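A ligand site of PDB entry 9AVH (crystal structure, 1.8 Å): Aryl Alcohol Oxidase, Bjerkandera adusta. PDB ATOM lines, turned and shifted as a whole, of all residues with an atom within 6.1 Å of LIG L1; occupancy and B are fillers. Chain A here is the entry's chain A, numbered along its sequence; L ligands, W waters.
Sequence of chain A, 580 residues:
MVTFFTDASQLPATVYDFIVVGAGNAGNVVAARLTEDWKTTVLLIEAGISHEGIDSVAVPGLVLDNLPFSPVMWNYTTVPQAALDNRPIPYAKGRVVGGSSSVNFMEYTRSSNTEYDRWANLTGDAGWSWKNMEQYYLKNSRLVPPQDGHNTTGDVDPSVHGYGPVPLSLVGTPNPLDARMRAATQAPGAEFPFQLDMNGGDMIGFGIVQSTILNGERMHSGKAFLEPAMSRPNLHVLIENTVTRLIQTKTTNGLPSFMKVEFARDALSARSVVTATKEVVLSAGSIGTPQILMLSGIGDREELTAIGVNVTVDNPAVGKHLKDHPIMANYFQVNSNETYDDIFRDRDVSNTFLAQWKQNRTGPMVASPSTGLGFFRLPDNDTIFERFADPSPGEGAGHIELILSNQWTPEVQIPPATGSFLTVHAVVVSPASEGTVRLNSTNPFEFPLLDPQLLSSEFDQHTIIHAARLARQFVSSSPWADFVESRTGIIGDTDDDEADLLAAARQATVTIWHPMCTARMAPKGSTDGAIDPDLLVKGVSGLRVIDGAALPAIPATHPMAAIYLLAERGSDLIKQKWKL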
ATOM      1  N   PHE A 105       2.421  13.293 -16.555  1.00  0.00           N
ATOM      2  CA  PHE A 105       2.247  14.727 -16.444  1.00  0.00           C
ATOM      3  C   PHE A 105       1.399  15.142 -15.246  1.00  0.00           C
ATOM      4  O   PHE A 105       0.987  16.314 -15.164  1.00  0.00           O
ATOM      5  CB  PHE A 105       1.735  15.213 -17.800  1.00  0.00           C
ATOM      6  CG  PHE A 105       2.715  15.036 -18.958  1.00  0.00           C
ATOM      7  CD1 PHE A 105       4.046  14.703 -18.751  1.00  0.00           C
ATOM      8  CD2 PHE A 105       2.301  15.180 -20.264  1.00  0.00           C
ATOM      9  CE1 PHE A 105       4.910  14.532 -19.815  1.00  0.00           C
ATOM     10  CE2 PHE A 105       3.173  14.961 -21.338  1.00  0.00           C
ATOM     11  CZ  PHE A 105       4.490  14.670 -21.101  1.00  0.00           C
ATOM     12  N   MET A 106       1.148  14.201 -14.329  1.00  0.00           N
ATOM     13  CA  MET A 106       0.648  14.491 -13.001  1.00  0.00           C
ATOM     14  C   MET A 106      -0.815  14.919 -12.937  1.00  0.00           C
ATOM     15  O   MET A 106      -1.265  15.299 -11.880  1.00  0.00           O
ATOM     16  CB  MET A 106       1.564  15.535 -12.322  1.00  0.00           C
ATOM     17  CG  MET A 106       2.939  14.955 -12.092  1.00  0.00           C
ATOM     18  SD  MET A 106       4.218  16.203 -11.831  1.00  0.00           S
ATOM     19  CE  MET A 106       4.514  16.671 -13.553  1.00  0.00           C
ATOM     20  N   GLU A 107      -1.595  14.786 -14.028  1.00  0.00           N
ATOM     21  CA  GLU A 107      -2.932  15.361 -14.056  1.00  0.00           C
ATOM     22  C   GLU A 107      -3.901  14.280 -13.606  1.00  0.00           C
ATOM     23  O   GLU A 107      -3.917  13.191 -14.183  1.00  0.00           O
ATOM     24  CB  GLU A 107      -3.291  15.937 -15.417  1.00  0.00           C
ATOM     25  CG  GLU A 107      -2.191  16.756 -16.095  1.00  0.00           C
ATOM     26  CD  GLU A 107      -1.564  17.927 -15.321  1.00  0.00           C
ATOM     27  OE1 GLU A 107      -0.963  18.822 -16.001  1.00  0.00           O
ATOM     28  OE2 GLU A 107      -1.687  17.956 -14.081  1.00  0.00           O
ATOM     29  N   ILE A 327      -3.344  12.524 -29.943  1.00  0.00           N
ATOM     30  CA  ILE A 327      -3.186  13.933 -29.609  1.00  0.00           C
ATOM     31  C   ILE A 327      -2.461  14.614 -30.757  1.00  0.00           C
ATOM     32  O   ILE A 327      -1.576  14.015 -31.375  1.00  0.00           O
ATOM     33  CB  ILE A 327      -2.433  14.097 -28.279  1.00  0.00           C
ATOM     34  CG1 ILE A 327      -2.245  15.553 -27.887  1.00  0.00           C
ATOM     35  CG2 ILE A 327      -1.085  13.386 -28.315  1.00  0.00           C
ATOM     36  CD1 ILE A 327      -1.838  15.690 -26.421  1.00  0.00           C
ATOM     37  N   PRO A 369       2.926  20.255 -16.833  1.00  0.00           N
ATOM     38  CA  PRO A 369       2.946  20.679 -18.241  1.00  0.00           C
ATOM     39  C   PRO A 369       1.633  21.235 -18.810  1.00  0.00           C
ATOM     40  O   PRO A 369       1.571  21.515 -19.993  1.00  0.00           O
ATOM     41  CB  PRO A 369       3.343  19.432 -19.021  1.00  0.00           C
ATOM     42  CG  PRO A 369       3.731  18.416 -18.004  1.00  0.00           C
ATOM     43  CD  PRO A 369       3.086  18.802 -16.700  1.00  0.00           C
ATOM     44  N   SER A 370       0.601  21.413 -17.994  1.00  0.00           N
ATOM     45  CA  SER A 370      -0.606  22.006 -18.516  1.00  0.00           C
ATOM     46  C   SER A 370      -1.179  22.899 -17.435  1.00  0.00           C
ATOM     47  O   SER A 370      -0.826  22.706 -16.277  1.00  0.00           O
ATOM     48  CB  SER A 370      -1.606  20.976 -18.999  1.00  0.00           C
ATOM     49  OG  SER A 370      -2.241  20.318 -17.906  1.00  0.00           O
ATOM     50  N   LEU A 373      -7.708  22.208 -18.576  1.00  0.00           N
ATOM     51  CA  LEU A 373      -8.207  21.115 -19.392  1.00  0.00           C
ATOM     52  C   LEU A 373      -9.648  21.430 -19.735  1.00  0.00           C
ATOM     53  O   LEU A 373     -10.423  21.742 -18.855  1.00  0.00           O
ATOM     54  CB  LEU A 373      -8.173  19.796 -18.623  1.00  0.00           C
ATOM     55  CG  LEU A 373      -6.873  19.397 -17.936  1.00  0.00           C
ATOM     56  CD1 LEU A 373      -7.066  18.084 -17.226  1.00  0.00           C
ATOM     57  CD2 LEU A 373      -5.683  19.252 -18.898  1.00  0.00           C
ATOM     58  N   ILE A 403      -6.195  20.724 -24.180  1.00  0.00           N
ATOM     59  CA  ILE A 403      -5.259  20.938 -23.090  1.00  0.00           C
ATOM     60  C   ILE A 403      -4.469  22.202 -23.350  1.00  0.00           C
ATOM     61  O   ILE A 403      -3.880  22.350 -24.416  1.00  0.00           O
ATOM     62  CB  ILE A 403      -4.299  19.735 -22.994  1.00  0.00           C
ATOM     63  CG1 ILE A 403      -5.052  18.405 -22.901  1.00  0.00           C
ATOM     64  CG2 ILE A 403      -3.317  19.930 -21.825  1.00  0.00           C
ATOM     65  CD1 ILE A 403      -4.163  17.187 -22.775  1.00  0.00           C
ATOM     66  N   LEU A 404      -4.458  23.099 -22.373  1.00  0.00           N
ATOM     67  CA  LEU A 404      -3.748  24.362 -22.480  1.00  0.00           C
ATOM     68  C   LEU A 404      -2.405  24.195 -21.796  1.00  0.00           C
ATOM     69  O   LEU A 404      -2.325  23.760 -20.645  1.00  0.00           O
ATOM     70  CB  LEU A 404      -4.506  25.498 -21.808  1.00  0.00           C
ATOM     71  CG  LEU A 404      -5.970  25.666 -22.211  1.00  0.00           C
ATOM     72  CD1 LEU A 404      -6.595  26.835 -21.415  1.00  0.00           C
ATOM     73  CD2 LEU A 404      -6.099  25.861 -23.707  1.00  0.00           C
ATOM     74  N   SER A 405      -1.357  24.585 -22.525  1.00  0.00           N
ATOM     75  CA  SER A 405       0.006  24.539 -22.041  1.00  0.00           C
ATOM     76  C   SER A 405       0.701  25.878 -22.254  1.00  0.00           C
ATOM     77  O   SER A 405       0.650  26.429 -23.372  1.00  0.00           O
ATOM     78  CB  SER A 405       0.799  23.436 -22.720  1.00  0.00           C
ATOM     79  OG  SER A 405       0.280  22.152 -22.420  1.00  0.00           O
ATOM     80  N   THR A 409       4.720  22.785 -26.314  1.00  0.00           N
ATOM     81  CA  THR A 409       4.954  21.442 -25.785  1.00  0.00           C
ATOM     82  C   THR A 409       5.577  20.630 -26.908  1.00  0.00           C
ATOM     83  O   THR A 409       4.947  20.481 -27.951  1.00  0.00           O
ATOM     84  CB  THR A 409       3.655  20.767 -25.327  1.00  0.00           C
ATOM     85  OG1 THR A 409       2.931  21.661 -24.496  1.00  0.00           O
ATOM     86  CG2 THR A 409       3.933  19.470 -24.589  1.00  0.00           C
ATOM     87  N   GLU A 411       6.181  17.630 -29.246  1.00  0.00           N
ATOM     88  CA  GLU A 411       5.528  16.387 -29.619  1.00  0.00           C
ATOM     89  C   GLU A 411       6.248  15.891 -30.869  1.00  0.00           C
ATOM     90  O   GLU A 411       7.388  15.463 -30.776  1.00  0.00           O
ATOM     91  CB  GLU A 411       4.035  16.603 -29.822  1.00  0.00           C
ATOM     92  CG  GLU A 411       3.267  16.560 -28.505  1.00  0.00           C
ATOM     93  CD  GLU A 411       1.782  16.875 -28.614  1.00  0.00           C
ATOM     94  OE1 GLU A 411       1.214  16.901 -29.732  1.00  0.00           O
ATOM     95  OE2 GLU A 411       1.246  17.126 -27.515  1.00  0.00           O
ATOM     96  N   HIS A 425      -3.577  21.471 -27.082  1.00  0.00           N
ATOM     97  CA  HIS A 425      -3.547  20.117 -27.595  1.00  0.00           C
ATOM     98  C   HIS A 425      -4.964  19.658 -27.868  1.00  0.00           C
ATOM     99  O   HIS A 425      -5.827  19.843 -27.020  1.00  0.00           O
ATOM    100  CB  HIS A 425      -2.894  19.145 -26.600  1.00  0.00           C
ATOM    101  CG  HIS A 425      -1.531  19.548 -26.135  1.00  0.00           C
ATOM    102  ND1 HIS A 425      -0.386  19.023 -26.701  1.00  0.00           N
ATOM    103  CD2 HIS A 425      -1.130  20.371 -25.165  1.00  0.00           C
ATOM    104  CE1 HIS A 425       0.658  19.547 -26.099  1.00  0.00           C
ATOM    105  NE2 HIS A 425       0.243  20.345 -25.142  1.00  0.00           N
ATOM    106  N   ILE A 512      -0.723   9.843 -26.910  1.00  0.00           N
ATOM    107  CA  ILE A 512      -0.532  10.495 -25.635  1.00  0.00           C
ATOM    108  C   ILE A 512       0.065   9.505 -24.635  1.00  0.00           C
ATOM    109  O   ILE A 512       0.403   9.880 -23.528  1.00  0.00           O
ATOM    110  CB  ILE A 512      -1.906  11.044 -25.192  1.00  0.00           C
ATOM    111  CG1 ILE A 512      -1.791  12.248 -24.372  1.00  0.00           C
ATOM    112  CG2 ILE A 512      -2.767   9.977 -24.500  1.00  0.00           C
ATOM    113  CD1 ILE A 512      -3.155  12.866 -24.103  1.00  0.00           C
ATOM    114  N   TRP A 513       0.159   8.228 -25.015  1.00  0.00           N
ATOM    115  CA  TRP A 513       0.689   7.169 -24.151  1.00  0.00           C
ATOM    116  C   TRP A 513      -0.259   6.782 -23.004  1.00  0.00           C
ATOM    117  O   TRP A 513       0.153   6.674 -21.860  1.00  0.00           O
ATOM    118  CB  TRP A 513       2.068   7.587 -23.609  1.00  0.00           C
ATOM    119  CG  TRP A 513       3.055   7.972 -24.684  1.00  0.00           C
ATOM    120  CD1 TRP A 513       3.312   7.326 -25.850  1.00  0.00           C
ATOM    121  CD2 TRP A 513       3.906   9.130 -24.673  1.00  0.00           C
ATOM    122  NE1 TRP A 513       4.295   7.969 -26.545  1.00  0.00           N
ATOM    123  CE2 TRP A 513       4.682   9.091 -25.863  1.00  0.00           C
ATOM    124  CE3 TRP A 513       4.067  10.211 -23.802  1.00  0.00           C
ATOM    125  CZ2 TRP A 513       5.612  10.061 -26.186  1.00  0.00           C
ATOM    126  CZ3 TRP A 513       4.980  11.203 -24.140  1.00  0.00           C
ATOM    127  CH2 TRP A 513       5.733  11.134 -25.327  1.00  0.00           C
ATOM    128  N   HIS A 514      -1.522   6.497 -23.355  1.00  0.00           N
ATOM    129  CA  HIS A 514      -2.533   5.961 -22.458  1.00  0.00           C
ATOM    130  C   HIS A 514      -3.007   4.617 -22.988  1.00  0.00           C
ATOM    131  O   HIS A 514      -4.207   4.377 -23.094  1.00  0.00           O
ATOM    132  CB  HIS A 514      -3.720   6.937 -22.345  1.00  0.00           C
ATOM    133  CG  HIS A 514      -3.406   8.262 -21.828  1.00  0.00           C
ATOM    134  ND1 HIS A 514      -4.351   9.257 -21.914  1.00  0.00           N
ATOM    135  CD2 HIS A 514      -2.307   8.805 -21.255  1.00  0.00           C
ATOM    136  CE1 HIS A 514      -3.840  10.372 -21.391  1.00  0.00           C
ATOM    137  NE2 HIS A 514      -2.609  10.151 -21.017  1.00  0.00           N
ATOM    138  N   HIS A 558      -7.524  11.652 -18.823  1.00  0.00           N
ATOM    139  CA  HIS A 558      -6.276  11.171 -18.260  1.00  0.00           C
ATOM    140  C   HIS A 558      -6.570   9.982 -17.349  1.00  0.00           C
ATOM    141  O   HIS A 558      -7.388  10.114 -16.452  1.00  0.00           O
ATOM    142  CB  HIS A 558      -5.620  12.316 -17.463  1.00  0.00           C
ATOM    143  CG  HIS A 558      -5.552  13.577 -18.242  1.00  0.00           C
ATOM    144  ND1 HIS A 558      -4.529  13.823 -19.103  1.00  0.00           N
ATOM    145  CD2 HIS A 558      -6.360  14.630 -18.312  1.00  0.00           C
ATOM    146  CE1 HIS A 558      -4.743  14.989 -19.718  1.00  0.00           C
ATOM    147  NE2 HIS A 558      -5.872  15.483 -19.269  1.00  0.00           N
ATOM    148  N   PRO A 559      -5.982   8.793 -17.605  1.00  0.00           N
ATOM    149  CA  PRO A 559      -6.406   7.561 -16.933  1.00  0.00           C
ATOM    150  C   PRO A 559      -5.834   7.158 -15.567  1.00  0.00           C
ATOM    151  O   PRO A 559      -6.291   6.165 -15.005  1.00  0.00           O
ATOM    152  CB  PRO A 559      -6.020   6.514 -17.994  1.00  0.00           C
ATOM    153  CG  PRO A 559      -4.746   7.059 -18.551  1.00  0.00           C
ATOM    154  CD  PRO A 559      -5.061   8.529 -18.724  1.00  0.00           C
HETATM  155  C1  LIG L   1       0.774  18.745 -22.337  1.00  0.00           C
HETATM  156  O1  LIG L   1      -0.175  18.437 -21.276  1.00  0.00           O
HETATM  157  C2  LIG L   1      -0.516  17.142 -21.136  1.00  0.00           C
HETATM  158  C3  LIG L   1      -1.052  16.752 -19.899  1.00  0.00           C
HETATM  159  C4  LIG L   1      -1.410  15.416 -19.680  1.00  0.00           C
HETATM  160  C5  LIG L   1      -1.202  14.490 -20.730  1.00  0.00           C
HETATM  161  C6  LIG L   1      -0.678  14.913 -21.933  1.00  0.00           C
HETATM  162  C7  LIG L   1      -0.339  16.235 -22.197  1.00  0.00           C
HETATM  163  C8  LIG L   1      -1.503  13.128 -20.542  1.00  0.00           C
HETATM  164  O2  LIG L   1      -2.431  12.763 -19.779  1.00  0.00           O
HETATM  165  O3  LIG L   1      -0.779  12.268 -21.094  1.00  0.00           O
HETATM  166  P1  LG2 L   2       2.447   1.493 -15.035  1.00  0.00           P
HETATM  167  O1  LG2 L   2       2.335   2.559 -14.010  1.00  0.00           O
HETATM  168  O2  LG2 L   2       3.190   1.775 -16.279  1.00  0.00           O
HETATM  169  O3  LG2 L   2       3.094   0.311 -14.184  1.00  0.00           O
HETATM  170  C1  LG2 L   2       3.643  -0.852 -14.814  1.00  0.00           C
HETATM  171  C2  LG2 L   2       4.853  -1.259 -14.039  1.00  0.00           C
HETATM  172  O4  LG2 L   2       5.207  -2.645 -14.309  1.00  0.00           O
HETATM  173  C3  LG2 L   2       6.078  -0.405 -14.384  1.00  0.00           C
HETATM  174  O5  LG2 L   2       6.675  -0.004 -13.145  1.00  0.00           O
HETATM  175  C4  LG2 L   2       6.886  -1.349 -15.273  1.00  0.00           C
HETATM  176  O6  LG2 L   2       8.273  -1.102 -15.267  1.00  0.00           O
HETATM  177  C5  LG2 L   2       6.591  -2.699 -14.643  1.00  0.00           C
HETATM  178  N1  LG2 L   2       6.764  -3.836 -15.534  1.00  0.00           N
HETATM  179  C6  LG2 L   2       6.312  -3.985 -16.824  1.00  0.00           C
HETATM  180  N2  LG2 L   2       6.591  -5.163 -17.356  1.00  0.00           N
HETATM  181  C7  LG2 L   2       7.234  -5.849 -16.323  1.00  0.00           C
HETATM  182  C8  LG2 L   2       7.770  -7.145 -16.235  1.00  0.00           C
HETATM  183  N3  LG2 L   2       7.729  -8.039 -17.231  1.00  0.00           N
HETATM  184  N4  LG2 L   2       8.350  -7.499 -15.062  1.00  0.00           N
HETATM  185  C9  LG2 L   2       8.391  -6.605 -14.066  1.00  0.00           C
HETATM  186  N5  LG2 L   2       7.915  -5.364 -14.036  1.00  0.00           N
HETATM  187  C10 LG2 L   2       7.345  -5.036 -15.198  1.00  0.00           C
HETATM  188  N6  LG2 L   2      -2.183   9.715 -17.092  1.00  0.00           N
HETATM  189  C11 LG2 L   2      -2.846  10.636 -16.335  1.00  0.00           C
HETATM  190  O7  LG2 L   2      -3.915  10.388 -15.799  1.00  0.00           O
HETATM  191  N7  LG2 L   2      -2.333  11.923 -16.259  1.00  0.00           N
HETATM  192  C12 LG2 L   2      -1.256  12.430 -16.979  1.00  0.00           C
HETATM  193  O8  LG2 L   2      -0.842  13.551 -16.744  1.00  0.00           O
HETATM  194  C13 LG2 L   2      -0.520  11.430 -17.689  1.00  0.00           C
HETATM  195  N8  LG2 L   2       0.584  11.798 -18.355  1.00  0.00           N
HETATM  196  C14 LG2 L   2       1.346  10.798 -18.894  1.00  0.00           C
HETATM  197  C15 LG2 L   2       2.609  11.114 -19.441  1.00  0.00           C
HETATM  198  C16 LG2 L   2       3.471  10.121 -19.860  1.00  0.00           C
HETATM  199  C17 LG2 L   2       4.873  10.476 -20.327  1.00  0.00           C
HETATM  200  C18 LG2 L   2       3.076   8.778 -19.733  1.00  0.00           C
HETATM  201  C19 LG2 L   2       4.015   7.675 -20.155  1.00  0.00           C
HETATM  202  C20 LG2 L   2       1.802   8.471 -19.349  1.00  0.00           C
HETATM  203  C21 LG2 L   2       0.931   9.442 -18.837  1.00  0.00           C
HETATM  204  N9  LG2 L   2      -0.335   9.121 -18.328  1.00  0.00           N
HETATM  205  C22 LG2 L   2      -1.072  10.093 -17.685  1.00  0.00           C
HETATM  206  C23 LG2 L   2      -0.854   7.749 -18.297  1.00  0.00           C
HETATM  207  C24 LG2 L   2      -0.766   7.013 -16.968  1.00  0.00           C
HETATM  208  O9  LG2 L   2       0.449   7.463 -16.366  1.00  0.00           O
HETATM  209  C25 LG2 L   2      -0.852   5.518 -17.242  1.00  0.00           C
HETATM  210  O10 LG2 L   2      -2.033   5.189 -17.999  1.00  0.00           O
HETATM  211  C26 LG2 L   2      -0.869   4.743 -15.911  1.00  0.00           C
HETATM  212  O11 LG2 L   2       0.063   5.301 -14.957  1.00  0.00           O
HETATM  213  C27 LG2 L   2      -0.536   3.266 -16.107  1.00  0.00           C
HETATM  214  O12 LG2 L   2      -0.761   2.588 -14.852  1.00  0.00           O
HETATM  215  P2  LG2 L   2      -0.429   1.018 -14.770  1.00  0.00           P
HETATM  216  O13 LG2 L   2      -1.361   0.294 -15.683  1.00  0.00           O
HETATM  217  O14 LG2 L   2      -0.347   0.692 -13.328  1.00  0.00           O
HETATM  218  O15 LG2 L   2       1.004   0.920 -15.423  1.00  0.00           O
HETATM  219  O   HOH W   1       1.479  12.235 -22.508  1.00  0.00           O
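A nitrogen (N8) of LG2 L2 lies close to an oxygen (O3) of LIG L1, 3.1 Å away.
Merely in contact with LIG L1: His 425, Phe 105, Ile 512, Ser 405, Ile 403, Ser 370, Pro 369, Glu 107 and Thr 409. The nearest printed residue that does not touch LIG L1 is Ile 327 (4.5 Å).
The side-chain carboxylate (OE1) of Glu 107 is in hydrogen-bond range of the side-chain hydroxyl (OG) of Ser 370. OG of Ser 405 sits at hydrogen-bond distance from O of Pro 369 (2.8 Å). A ring nitrogen (NE2) of His 425 sits at hydrogen-bond distance from the side-chain hydroxyl (OG1) of Thr 409 (3.1 Å). A ring nitrogen (ND1) of His 425 lies within hydrogen-bond range of the side-chain carboxylate of Glu 411, 2.6 Å away. OG1 of Thr 409 lies close to OG of Ser 405 (3.4 Å). The side-chain hydroxyl (OG) of Ser 405 is in hydrogen-bond range of a ring nitrogen (NE2) of His 425 (3.3 Å). N of His 425 lies within hydrogen-bond range of O of Ile 403, at 2.8 Å.
The backbone carbonyl oxygen of Glu 107 lies within hydrogen-bond range of a nitrogen (N7) of LG2 L2. The backbone NH (N) of Glu 107 sits at hydrogen-bond distance from an oxygen (O8) of LG2 L2 (3.1 Å). N of Met 106 sits at hydrogen-bond distance from O8 of LG2 L2, 3.2 Å away. A ring nitrogen (NE2) of His 514 lies within hydrogen-bond range of an oxygen (O3) of LIG L1. ND1 of His 558 is in hydrogen-bond range of O2 of LIG L1 (2.4 Å). N of Phe 105 lies within hydrogen-bond range of N8 of LG2 L2 (3.0 Å).
Water W1 lies within hydrogen-bond range of an oxygen (O3) of LIG L1 (2.7 Å) and the backbone carbonyl oxygen of Ile 512 (2.8 Å).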
